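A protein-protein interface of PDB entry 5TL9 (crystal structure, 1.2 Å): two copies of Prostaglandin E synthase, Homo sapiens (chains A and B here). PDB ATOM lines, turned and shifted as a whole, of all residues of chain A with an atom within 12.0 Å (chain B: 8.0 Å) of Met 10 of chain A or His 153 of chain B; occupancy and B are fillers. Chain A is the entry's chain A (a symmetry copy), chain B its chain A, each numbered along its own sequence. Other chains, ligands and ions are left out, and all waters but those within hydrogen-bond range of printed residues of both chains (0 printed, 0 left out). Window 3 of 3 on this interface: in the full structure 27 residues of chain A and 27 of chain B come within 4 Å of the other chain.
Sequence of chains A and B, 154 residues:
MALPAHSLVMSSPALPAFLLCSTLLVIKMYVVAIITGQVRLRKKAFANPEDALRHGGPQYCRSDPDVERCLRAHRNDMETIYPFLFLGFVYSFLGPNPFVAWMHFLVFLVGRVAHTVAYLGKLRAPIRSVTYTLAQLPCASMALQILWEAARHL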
ATOM      1  N   SER A   7     -32.448  19.712  26.944  1.00  0.00           N
ATOM      2  CA  SER A   7     -31.363  20.348  26.140  1.00  0.00           C
ATOM      3  C   SER A   7     -30.219  19.375  25.864  1.00  0.00           C
ATOM      4  O   SER A   7     -29.860  18.562  26.724  1.00  0.00           O
ATOM      5  CB  SER A   7     -30.834  21.599  26.847  1.00  0.00           C
ATOM      6  OG  SER A   7     -29.809  22.231  26.093  1.00  0.00           O
ATOM      7  N   LEU A   8     -29.646  19.484  24.666  1.00  0.00           N
ATOM      8  CA  LEU A   8     -28.535  18.627  24.234  1.00  0.00           C
ATOM      9  C   LEU A   8     -27.172  19.042  24.811  1.00  0.00           C
ATOM     10  O   LEU A   8     -26.164  18.370  24.581  1.00  0.00           O
ATOM     11  CB  LEU A   8     -28.494  18.514  22.699  1.00  0.00           C
ATOM     12  CG  LEU A   8     -29.694  17.824  22.022  1.00  0.00           C
ATOM     13  CD1 LEU A   8     -29.719  18.063  20.522  1.00  0.00           C
ATOM     14  CD2 LEU A   8     -29.760  16.327  22.314  1.00  0.00           C
ATOM     15  N   VAL A   9     -27.162  20.139  25.573  1.00  0.00           N
ATOM     16  CA  VAL A   9     -25.996  20.576  26.364  1.00  0.00           C
ATOM     17  C   VAL A   9     -25.654  19.566  27.477  1.00  0.00           C
ATOM     18  O   VAL A   9     -24.489  19.461  27.889  1.00  0.00           O
ATOM     19  CB  VAL A   9     -26.202  22.010  26.927  1.00  0.00           C
ATOM     20  CG1 VAL A   9     -25.005  22.492  27.738  1.00  0.00           C
ATOM     21  CG2 VAL A   9     -26.443  22.985  25.789  1.00  0.00           C
ATOM     22  N   MET A  10     -26.658  18.827  27.945  1.00  0.00           N
ATOM     23  CA  MET A  10     -26.466  17.798  28.969  1.00  0.00           C
ATOM     24  C   MET A  10     -26.231  16.391  28.406  1.00  0.00           C
ATOM     25  O   MET A  10     -26.515  15.389  29.076  1.00  0.00           O
ATOM     26  CB  MET A  10     -27.637  17.806  29.951  1.00  0.00           C
ATOM     27  CG  MET A  10     -27.462  18.804  31.078  1.00  0.00           C
ATOM     28  SD  MET A  10     -28.855  18.818  32.214  1.00  0.00           S
ATOM     29  CE  MET A  10     -28.565  17.332  33.175  1.00  0.00           C
ATOM     30  N   SER A  11     -25.690  16.329  27.188  1.00  0.00           N
ATOM     31  CA  SER A  11     -25.366  15.052  26.522  1.00  0.00           C
ATOM     32  C   SER A  11     -24.259  14.293  27.255  1.00  0.00           C
ATOM     33  O   SER A  11     -24.194  13.061  27.196  1.00  0.00           O
ATOM     34  CB  SER A  11     -24.971  15.284  25.063  1.00  0.00           C
ATOM     35  OG  SER A  11     -26.076  15.737  24.302  1.00  0.00           O
ATOM     36  N   SER A  12     -23.397  15.048  27.935  1.00  0.00           N
ATOM     37  CA  SER A  12     -22.375  14.515  28.825  1.00  0.00           C
ATOM     38  C   SER A  12     -22.142  15.501  29.980  1.00  0.00           C
ATOM     39  O   SER A  12     -22.286  16.710  29.779  1.00  0.00           O
ATOM     40  CB  SER A  12     -21.082  14.252  28.050  1.00  0.00           C
ATOM     41  OG  SER A  12     -20.480  15.457  27.616  1.00  0.00           O
ATOM     42  N   PRO A  13     -21.783  14.994  31.188  1.00  0.00           N
ATOM     43  CA  PRO A  13     -21.586  15.868  32.359  1.00  0.00           C
ATOM     44  C   PRO A  13     -20.562  16.998  32.177  1.00  0.00           C
ATOM     45  O   PRO A  13     -20.725  18.059  32.775  1.00  0.00           O
ATOM     46  CB  PRO A  13     -21.118  14.895  33.447  1.00  0.00           C
ATOM     47  CG  PRO A  13     -21.728  13.595  33.061  1.00  0.00           C
ATOM     48  CD  PRO A  13     -21.679  13.566  31.563  1.00  0.00           C
ATOM     49  N   ALA A  14     -19.532  16.768  31.361  1.00  0.00           N
ATOM     50  CA  ALA A  14     -18.456  17.745  31.133  1.00  0.00           C
ATOM     51  C   ALA A  14     -18.790  18.803  30.079  1.00  0.00           C
ATOM     52  O   ALA A  14     -18.116  19.844  29.994  1.00  0.00           O
ATOM     53  CB  ALA A  14     -17.179  17.016  30.744  1.00  0.00           C
ATOM     54  N   LEU A  15     -19.815  18.534  29.275  1.00  0.00           N
ATOM     55  CA  LEU A  15     -20.122  19.367  28.115  1.00  0.00           C
ATOM     56  C   LEU A  15     -20.454  20.836  28.433  1.00  0.00           C
ATOM     57  O   LEU A  15     -19.921  21.713  27.757  1.00  0.00           O
ATOM     58  CB  LEU A  15     -21.182  18.720  27.206  1.00  0.00           C
ATOM     59  CG  LEU A  15     -21.413  19.346  25.822  1.00  0.00           C
ATOM     60  CD1 LEU A  15     -20.179  19.260  24.926  1.00  0.00           C
ATOM     61  CD2 LEU A  15     -22.609  18.696  25.145  1.00  0.00           C
ATOM     62  N   PRO A  16     -21.311  21.116  29.449  1.00  0.00           N
ATOM     63  CA  PRO A  16     -21.577  22.530  29.755  1.00  0.00           C
ATOM     64  C   PRO A  16     -20.309  23.337  30.073  1.00  0.00           C
ATOM     65  O   PRO A  16     -20.150  24.447  29.548  1.00  0.00           O
ATOM     66  CB  PRO A  16     -22.508  22.454  30.973  1.00  0.00           C
ATOM     67  CG  PRO A  16     -23.223  21.161  30.801  1.00  0.00           C
ATOM     68  CD  PRO A  16     -22.178  20.229  30.257  1.00  0.00           C
ATOM     69  N   ALA A  17     -19.414  22.777  30.887  1.00  0.00           N
ATOM     70  CA  ALA A  17     -18.149  23.440  31.225  1.00  0.00           C
ATOM     71  C   ALA A  17     -17.285  23.680  29.986  1.00  0.00           C
ATOM     72  O   ALA A  17     -16.703  24.758  29.827  1.00  0.00           O
ATOM     73  CB  ALA A  17     -17.372  22.639  32.257  1.00  0.00           C
ATOM     74  N   PHE A  18     -17.212  22.676  29.111  1.00  0.00           N
ATOM     75  CA  PHE A  18     -16.477  22.812  27.863  1.00  0.00           C
ATOM     76  C   PHE A  18     -17.044  23.943  27.010  1.00  0.00           C
ATOM     77  O   PHE A  18     -16.290  24.769  26.501  1.00  0.00           O
ATOM     78  CB  PHE A  18     -16.459  21.515  27.050  1.00  0.00           C
ATOM     79  CG  PHE A  18     -15.977  21.725  25.641  1.00  0.00           C
ATOM     80  CD1 PHE A  18     -14.633  22.015  25.385  1.00  0.00           C
ATOM     81  CD2 PHE A  18     -16.882  21.732  24.573  1.00  0.00           C
ATOM     82  CE1 PHE A  18     -14.196  22.262  24.090  1.00  0.00           C
ATOM     83  CE2 PHE A  18     -16.449  21.982  23.275  1.00  0.00           C
ATOM     84  CZ  PHE A  18     -15.104  22.242  23.034  1.00  0.00           C
ATOM     85  N   LEU A  19     -18.366  23.956  26.848  1.00  0.00           N
ATOM     86  CA  LEU A  19     -19.021  24.948  26.002  1.00  0.00           C
ATOM     87  C   LEU A  19     -18.870  26.360  26.552  1.00  0.00           C
ATOM     88  O   LEU A  19     -18.686  27.303  25.783  1.00  0.00           O
ATOM     89  CB  LEU A  19     -20.490  24.587  25.760  1.00  0.00           C
ATOM     90  CG  LEU A  19     -20.745  23.327  24.920  1.00  0.00           C
ATOM     91  CD1 LEU A  19     -22.238  23.040  24.861  1.00  0.00           C
ATOM     92  CD2 LEU A  19     -20.162  23.424  23.516  1.00  0.00           C
ATOM     93  N   LEU A  20     -18.915  26.495  27.881  1.00  0.00           N
ATOM     94  CA  LEU A  20     -18.689  27.783  28.532  1.00  0.00           C
ATOM     95  C   LEU A  20     -17.273  28.297  28.263  1.00  0.00           C
ATOM     96  O   LEU A  20     -17.098  29.422  27.785  1.00  0.00           O
ATOM     97  CB  LEU A  20     -18.954  27.690  30.041  1.00  0.00           C
ATOM     98  CG  LEU A  20     -18.854  28.999  30.839  1.00  0.00           C
ATOM     99  CD1 LEU A  20     -20.163  29.774  30.804  1.00  0.00           C
ATOM    100  CD2 LEU A  20     -18.461  28.710  32.279  1.00  0.00           C
ATOM    101  N   CYS A  21     -16.270  27.468  28.559  1.00  0.00           N
ATOM    102  CA  CYS A  21     -14.873  27.871  28.389  1.00  0.00           C
ATOM    103  C   CYS A  21     -14.535  28.179  26.931  1.00  0.00           C
ATOM    104  O   CYS A  21     -13.885  29.187  26.643  1.00  0.00           O
ATOM    105  CB  CYS A  21     -13.927  26.815  28.954  1.00  0.00           C
ATOM    106  SG  CYS A  21     -14.016  26.666  30.750  1.00  0.00           S
ATOM    107  N   THR A  23     -16.600  29.042  24.395  1.00  0.00           N
ATOM    108  CA  THR A  23     -17.291  30.233  23.912  1.00  0.00           C
ATOM    109  C   THR A  23     -16.631  31.504  24.455  1.00  0.00           C
ATOM    110  O   THR A  23     -16.450  32.468  23.714  1.00  0.00           O
ATOM    111  CB  THR A  23     -18.801  30.168  24.190  1.00  0.00           C
ATOM    112  OG1 THR A  23     -19.316  28.953  23.631  1.00  0.00           O
ATOM    113  CG2 THR A  23     -19.522  31.340  23.548  1.00  0.00           C
ATOM    114  N   PHE A  89     -14.114  19.125  22.788  1.00  0.00           N
ATOM    115  CA  PHE A  89     -15.432  18.624  22.405  1.00  0.00           C
ATOM    116  C   PHE A  89     -15.460  17.099  22.435  1.00  0.00           C
ATOM    117  O   PHE A  89     -16.339  16.503  23.064  1.00  0.00           O
ATOM    118  CB  PHE A  89     -15.858  19.159  21.031  1.00  0.00           C
ATOM    119  CG  PHE A  89     -17.240  18.729  20.618  1.00  0.00           C
ATOM    120  CD1 PHE A  89     -18.373  19.324  21.185  1.00  0.00           C
ATOM    121  CD2 PHE A  89     -17.417  17.716  19.671  1.00  0.00           C
ATOM    122  CE1 PHE A  89     -19.651  18.925  20.808  1.00  0.00           C
ATOM    123  CE2 PHE A  89     -18.694  17.311  19.293  1.00  0.00           C
ATOM    124  CZ  PHE A  89     -19.811  17.917  19.860  1.00  0.00           C
ATOM    125  N   SER A  92     -15.039  15.679  25.997  1.00  0.00           N
ATOM    126  CA  SER A  92     -16.281  15.789  26.769  1.00  0.00           C
ATOM    127  C   SER A  92     -17.165  14.542  26.663  1.00  0.00           C
ATOM    128  O   SER A  92     -17.919  14.241  27.589  1.00  0.00           O
ATOM    129  CB  SER A  92     -17.075  17.022  26.341  1.00  0.00           C
ATOM    130  OG  SER A  92     -16.412  18.212  26.727  1.00  0.00           O
ATOM    131  N   PHE A  93     -17.057  13.817  25.550  1.00  0.00           N
ATOM    132  CA  PHE A  93     -17.869  12.617  25.307  1.00  0.00           C
ATOM    133  C   PHE A  93     -17.191  11.286  25.650  1.00  0.00           C
ATOM    134  O   PHE A  93     -17.763  10.214  25.417  1.00  0.00           O
ATOM    135  CB  PHE A  93     -18.382  12.611  23.863  1.00  0.00           C
ATOM    136  CG  PHE A  93     -19.411  13.665  23.585  1.00  0.00           C
ATOM    137  CD1 PHE A  93     -20.748  13.468  23.941  1.00  0.00           C
ATOM    138  CD2 PHE A  93     -19.055  14.864  22.973  1.00  0.00           C
ATOM    139  CE1 PHE A  93     -21.705  14.439  23.688  1.00  0.00           C
ATOM    140  CE2 PHE A  93     -20.008  15.842  22.719  1.00  0.00           C
ATOM    141  CZ  PHE A  93     -21.337  15.631  23.076  1.00  0.00           C
ATOM    142  N   LEU A  94     -15.991  11.356  26.225  1.00  0.00           N
ATOM    143  CA  LEU A  94     -15.232  10.157  26.598  1.00  0.00           C
ATOM    144  C   LEU A  94     -15.500   9.717  28.039  1.00  0.00           C
ATOM    145  O   LEU A  94     -14.817   8.830  28.564  1.00  0.00           O
ATOM    146  CB  LEU A  94     -13.728  10.370  26.375  1.00  0.00           C
ATOM    147  CG  LEU A  94     -13.205  10.802  25.000  1.00  0.00           C
ATOM    148  CD1 LEU A  94     -11.689  10.864  25.044  1.00  0.00           C
ATOM    149  CD2 LEU A  94     -13.663   9.896  23.867  1.00  0.00           C
ATOM    150  N   GLY A  95     -16.507  10.336  28.653  1.00  0.00           N
ATOM    151  CA  GLY A  95     -16.871  10.102  30.051  1.00  0.00           C
ATOM    152  C   GLY A  95     -15.752  10.361  31.051  1.00  0.00           C
ATOM    153  O   GLY A  95     -15.478   9.492  31.885  1.00  0.00           O
ATOM    154  N   PRO A  96     -15.093  11.547  30.978  1.00  0.00           N
ATOM    155  CA  PRO A  96     -14.055  11.822  31.973  1.00  0.00           C
ATOM    156  C   PRO A  96     -14.679  12.210  33.316  1.00  0.00           C
ATOM    157  O   PRO A  96     -15.861  12.579  33.358  1.00  0.00           O
ATOM    158  CB  PRO A  96     -13.296  13.005  31.367  1.00  0.00           C
ATOM    159  CG  PRO A  96     -14.326  13.738  30.575  1.00  0.00           C
ATOM    160  CD  PRO A  96     -15.285  12.698  30.065  1.00  0.00           C
ATOM    161  N   PRO A  98     -15.906  14.479  36.031  1.00  0.00           N
ATOM    162  CA  PRO A  98     -16.410  15.853  35.900  1.00  0.00           C
ATOM    163  C   PRO A  98     -15.425  16.911  36.402  1.00  0.00           C
ATOM    164  O   PRO A  98     -15.127  17.859  35.669  1.00  0.00           O
ATOM    165  CB  PRO A  98     -17.687  15.842  36.746  1.00  0.00           C
ATOM    166  CG  PRO A  98     -18.156  14.432  36.674  1.00  0.00           C
ATOM    167  CD  PRO A  98     -16.904  13.604  36.682  1.00  0.00           C
ATOM    168  N   TRP A 102     -13.223  19.667  34.232  1.00  0.00           N
ATOM    169  CA  TRP A 102     -13.279  21.090  34.600  1.00  0.00           C
ATOM    170  C   TRP A 102     -11.889  21.694  34.749  1.00  0.00           C
ATOM    171  O   TRP A 102     -11.620  22.783  34.247  1.00  0.00           O
ATOM    172  CB  TRP A 102     -14.031  21.277  35.918  1.00  0.00           C
ATOM    173  CG  TRP A 102     -15.517  21.266  35.804  1.00  0.00           C
ATOM    174  CD1 TRP A 102     -16.279  20.416  35.060  1.00  0.00           C
ATOM    175  CD2 TRP A 102     -16.432  22.135  36.482  1.00  0.00           C
ATOM    176  NE1 TRP A 102     -17.612  20.699  35.230  1.00  0.00           N
ATOM    177  CE2 TRP A 102     -17.733  21.754  36.098  1.00  0.00           C
ATOM    178  CE3 TRP A 102     -16.279  23.201  37.374  1.00  0.00           C
ATOM    179  CZ2 TRP A 102     -18.872  22.403  36.569  1.00  0.00           C
ATOM    180  CZ3 TRP A 102     -17.411  23.843  37.842  1.00  0.00           C
ATOM    181  CH2 TRP A 102     -18.690  23.441  37.439  1.00  0.00           C
ATOM    182  N   PHE A 105     -10.290  22.208  31.335  1.00  0.00           N
ATOM    183  CA  PHE A 105     -10.871  23.362  30.648  1.00  0.00           C
ATOM    184  C   PHE A 105     -10.475  24.687  31.295  1.00  0.00           C
ATOM    185  O   PHE A 105     -10.171  25.647  30.587  1.00  0.00           O
ATOM    186  CB  PHE A 105     -12.401  23.257  30.559  1.00  0.00           C
ATOM    187  CG  PHE A 105     -12.912  21.959  29.976  1.00  0.00           C
ATOM    188  CD1 PHE A 105     -12.218  21.275  28.968  1.00  0.00           C
ATOM    189  CD2 PHE A 105     -14.129  21.436  30.413  1.00  0.00           C
ATOM    190  CE1 PHE A 105     -12.712  20.083  28.440  1.00  0.00           C
ATOM    191  CE2 PHE A 105     -14.628  20.250  29.887  1.00  0.00           C
ATOM    192  CZ  PHE A 105     -13.922  19.572  28.901  1.00  0.00           C
ATOM    193  N   LEU B  94     -29.246  23.844  20.061  1.00  0.00           N
ATOM    194  CA  LEU B  94     -29.868  24.575  21.172  1.00  0.00           C
ATOM    195  C   LEU B  94     -31.367  24.801  20.960  1.00  0.00           C
ATOM    196  O   LEU B  94     -32.005  25.544  21.715  1.00  0.00           O
ATOM    197  CB  LEU B  94     -29.154  25.912  21.416  1.00  0.00           C
ATOM    198  CG  LEU B  94     -27.643  25.944  21.671  1.00  0.00           C
ATOM    199  CD1 LEU B  94     -27.219  27.374  21.952  1.00  0.00           C
ATOM    200  CD2 LEU B  94     -27.201  25.030  22.803  1.00  0.00           C
ATOM    201  N   ILE B 146     -25.102  30.553  23.345  1.00  0.00           N
ATOM    202  CA  ILE B 146     -24.364  29.403  23.861  1.00  0.00           C
ATOM    203  C   ILE B 146     -23.905  29.655  25.298  1.00  0.00           C
ATOM    204  O   ILE B 146     -24.019  28.762  26.148  1.00  0.00           O
ATOM    205  CB  ILE B 146     -23.176  29.015  22.949  1.00  0.00           C
ATOM    206  CG1 ILE B 146     -23.683  28.579  21.567  1.00  0.00           C
ATOM    207  CG2 ILE B 146     -22.363  27.888  23.579  1.00  0.00           C
ATOM    208  CD1 ILE B 146     -22.638  28.598  20.471  1.00  0.00           C
ATOM    209  N   LEU B 147     -23.408  30.867  25.566  1.00  0.00           N
ATOM    210  CA  LEU B 147     -22.978  31.244  26.913  1.00  0.00           C
ATOM    211  C   LEU B 147     -24.076  31.029  27.938  1.00  0.00           C
ATOM    212  O   LEU B 147     -23.833  30.431  28.988  1.00  0.00           O
ATOM    213  CB  LEU B 147     -22.522  32.704  26.978  1.00  0.00           C
ATOM    214  CG  LEU B 147     -21.127  33.144  26.544  1.00  0.00           C
ATOM    215  CD1 LEU B 147     -20.967  34.604  26.927  1.00  0.00           C
ATOM    216  CD2 LEU B 147     -20.013  32.315  27.175  1.00  0.00           C
ATOM    217  N   TRP B 148     -25.284  31.511  27.628  1.00  0.00           N
ATOM    218  CA  TRP B 148     -26.407  31.394  28.565  1.00  0.00           C
ATOM    219  C   TRP B 148     -26.807  29.950  28.788  1.00  0.00           C
ATOM    220  O   TRP B 148     -27.052  29.549  29.930  1.00  0.00           O
ATOM    221  CB  TRP B 148     -27.635  32.200  28.122  1.00  0.00           C
ATOM    222  CG  TRP B 148     -27.390  33.617  27.684  1.00  0.00           C
ATOM    223  CD1 TRP B 148     -28.091  34.291  26.724  1.00  0.00           C
ATOM    224  CD2 TRP B 148     -26.391  34.531  28.169  1.00  0.00           C
ATOM    225  NE1 TRP B 148     -27.598  35.559  26.579  1.00  0.00           N
ATOM    226  CE2 TRP B 148     -26.554  35.738  27.449  1.00  0.00           C
ATOM    227  CE3 TRP B 148     -25.375  34.452  29.141  1.00  0.00           C
ATOM    228  CZ2 TRP B 148     -25.740  36.864  27.666  1.00  0.00           C
ATOM    229  CZ3 TRP B 148     -24.558  35.573  29.355  1.00  0.00           C
ATOM    230  CH2 TRP B 148     -24.751  36.761  28.619  1.00  0.00           C
ATOM    231  N   GLU B 149     -26.867  29.180  27.697  1.00  0.00           N
ATOM    232  CA  GLU B 149     -27.255  27.770  27.757  1.00  0.00           C
ATOM    233  C   GLU B 149     -26.224  26.950  28.518  1.00  0.00           C
ATOM    234  O   GLU B 149     -26.578  26.133  29.359  1.00  0.00           O
ATOM    235  CB  GLU B 149     -27.477  27.188  26.357  1.00  0.00           C
ATOM    236  CG  GLU B 149     -28.765  27.641  25.691  1.00  0.00           C
ATOM    237  CD  GLU B 149     -29.985  27.401  26.558  1.00  0.00           C
ATOM    238  OE1 GLU B 149     -30.799  28.334  26.700  1.00  0.00           O
ATOM    239  OE2 GLU B 149     -30.123  26.288  27.108  1.00  0.00           O
ATOM    240  N   ALA B 150     -24.942  27.176  28.226  1.00  0.00           N
ATOM    241  CA  ALA B 150     -23.870  26.472  28.922  1.00  0.00           C
ATOM    242  C   ALA B 150     -23.835  26.827  30.413  1.00  0.00           C
ATOM    243  O   ALA B 150     -23.826  25.929  31.264  1.00  0.00           O
ATOM    244  CB  ALA B 150     -22.525  26.749  28.263  1.00  0.00           C
ATOM    245  N   ALA B 151     -23.854  28.127  30.723  1.00  0.00           N
ATOM    246  CA  ALA B 151     -23.802  28.601  32.110  1.00  0.00           C
ATOM    247  C   ALA B 151     -24.956  28.058  32.952  1.00  0.00           C
ATOM    248  O   ALA B 151     -24.749  27.668  34.106  1.00  0.00           O
ATOM    249  CB  ALA B 151     -23.777  30.124  32.166  1.00  0.00           C
ATOM    250  N   ARG B 152     -26.154  28.000  32.371  1.00  0.00           N
ATOM    251  CA  ARG B 152     -27.340  27.580  33.123  1.00  0.00           C
ATOM    252  C   ARG B 152     -27.392  26.066  33.367  1.00  0.00           C
ATOM    253  O   ARG B 152     -28.175  25.609  34.200  1.00  0.00           O
ATOM    254  CB  ARG B 152     -28.631  28.113  32.483  1.00  0.00           C
ATOM    255  CG  ARG B 152     -29.178  27.314  31.313  1.00  0.00           C
ATOM    256  CD  ARG B 152     -30.385  28.004  30.697  1.00  0.00           C
ATOM    257  NE  ARG B 152     -31.158  27.102  29.843  1.00  0.00           N
ATOM    258  CZ  ARG B 152     -32.045  26.208  30.280  1.00  0.00           C
ATOM    259  NH1 ARG B 152     -32.302  26.085  31.579  1.00  0.00           N
ATOM    260  NH2 ARG B 152     -32.683  25.431  29.413  1.00  0.00           N
ATOM    261  N   HIS B 153     -26.548  25.310  32.655  1.00  0.00           N
ATOM    262  CA  HIS B 153     -26.467  23.856  32.815  1.00  0.00           C
ATOM    263  C   HIS B 153     -25.279  23.414  33.676  1.00  0.00           C
ATOM    264  O   HIS B 153     -25.020  22.212  33.818  1.00  0.00           O
ATOM    265  CB  HIS B 153     -26.436  23.163  31.448  1.00  0.00           C
ATOM    266  CG  HIS B 153     -27.764  23.129  30.759  1.00  0.00           C
ATOM    267  ND1 HIS B 153     -28.203  24.146  29.940  1.00  0.00           N
ATOM    268  CD2 HIS B 153     -28.748  22.200  30.764  1.00  0.00           C
ATOM    269  CE1 HIS B 153     -29.401  23.846  29.471  1.00  0.00           C
ATOM    270  NE2 HIS B 153     -29.754  22.670  29.956  1.00  0.00           N
ATOM    271  N   LEU B 154     -24.567  24.378  34.262  1.00  0.00           N
ATOM    272  CA  LEU B 154     -23.411  24.082  35.119  1.00  0.00           C
ATOM    273  C   LEU B 154     -23.824  23.477  36.457  1.00  0.00           C
ATOM    274  O   LEU B 154     -24.845  23.849  37.035  1.00  0.00           O
ATOM    275  CB  LEU B 154     -22.553  25.329  35.354  1.00  0.00           C
ATOM    276  CG  LEU B 154     -21.804  25.980  34.185  1.00  0.00           C
ATOM    277  CD1 LEU B 154     -21.193  27.297  34.640  1.00  0.00           C
ATOM    278  CD2 LEU B 154     -20.733  25.075  33.590  1.00  0.00           C
ATOM    279  OXT LEU B 154     -23.143  22.607  36.997  1.00  0.00           O
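CB of Ser 7 of chain A touches NE2 of His 153 of chain B, at 3.5 Å. Leu 94 of chain B touches Val 9 of chain A. Ala 150 of chain B touches Pro 16 of chain A. Pro 16 of chain A touches Leu 154 of chain B. CB of Ala 150 of chain B touches CB of Leu 19 of chain A (3.9 Å). Leu 20 of chain A touches Ala 150 of chain B. Leu 20 of chain A touches Ala 151 of chain B. CD2 of Leu 20 of chain A touches CD1 of Leu 154 of chain B, 3.9 Å away. OG1 of Thr 23 of chain A touches CG2 of Ile 146 of chain B, 3.2 Å away. CG2 of Thr 23 of chain A touches CD2 of Leu 147 of chain B (3.8 Å).
The backbone carbonyl oxygen (O) of Glu 149 of chain B lies within hydrogen-bond range of a ring nitrogen (ND1) of His 153 of chain B, at 2.6 Å. OG of Ser 7 of chain A sits close to N of Val 9 of chain A, at 3.4 Å. SG of Cys 21 of chain A is in hydrogen-bond range of O of Ala 17 of chain A (3.4 Å). The side-chain hydroxyl of Thr 23 of chain A lies within hydrogen-bond range of the backbone carbonyl oxygen of Leu 19 of chain A, at 2.8 Å.
Position printed for both chains: 94. Of the 13 pairs that touch across the chains among the printed residues, none has its exchanged pair printed and touching as well.
Of the printed residues of chain B, Met 10 of chain A touches His 153 (3.6 Å). Printed residues of chain A within 4 Å of His 153 of chain B: Ser 7 (3.5 Å), Met 10 (3.6 Å) and Pro 16 (3.7 Å). Of the printed residues of chain A, Ala 150 of chain B touches Pro 16, Leu 19 and Leu 20. Of chain A, only Leu 20 (3.9 Å) comes within 4 Å of Ala 151 of chain B. No residue of chain A comes within 4 Å of Arg 152 of chain B. Printed residues of chain B within 4 Å of Ser 7 of chain A: His 153. Of the printed residues of chain B, Leu 19 of chain A touches Ala 150 (3.9 Å). The nearest printed residue of chain B that does not touch Met 10 of chain A is Leu 154 of chain B (7.0 Å). The nearest printed residue of chain A that does not touch Leu 154 of chain B is Trp 102 of chain A (4.3 Å).
Of the 25 printed residues of chain A, 8 touch a printed residue of chain B. Hydrophobic or aromatic side chains of chain B that line the printed part of chain A: Leu 94, Ile 146, Leu 147, Ala 150, Ala 151, His 153 and Leu 154. Among the printed residues, 13 pairs touch across the chains.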
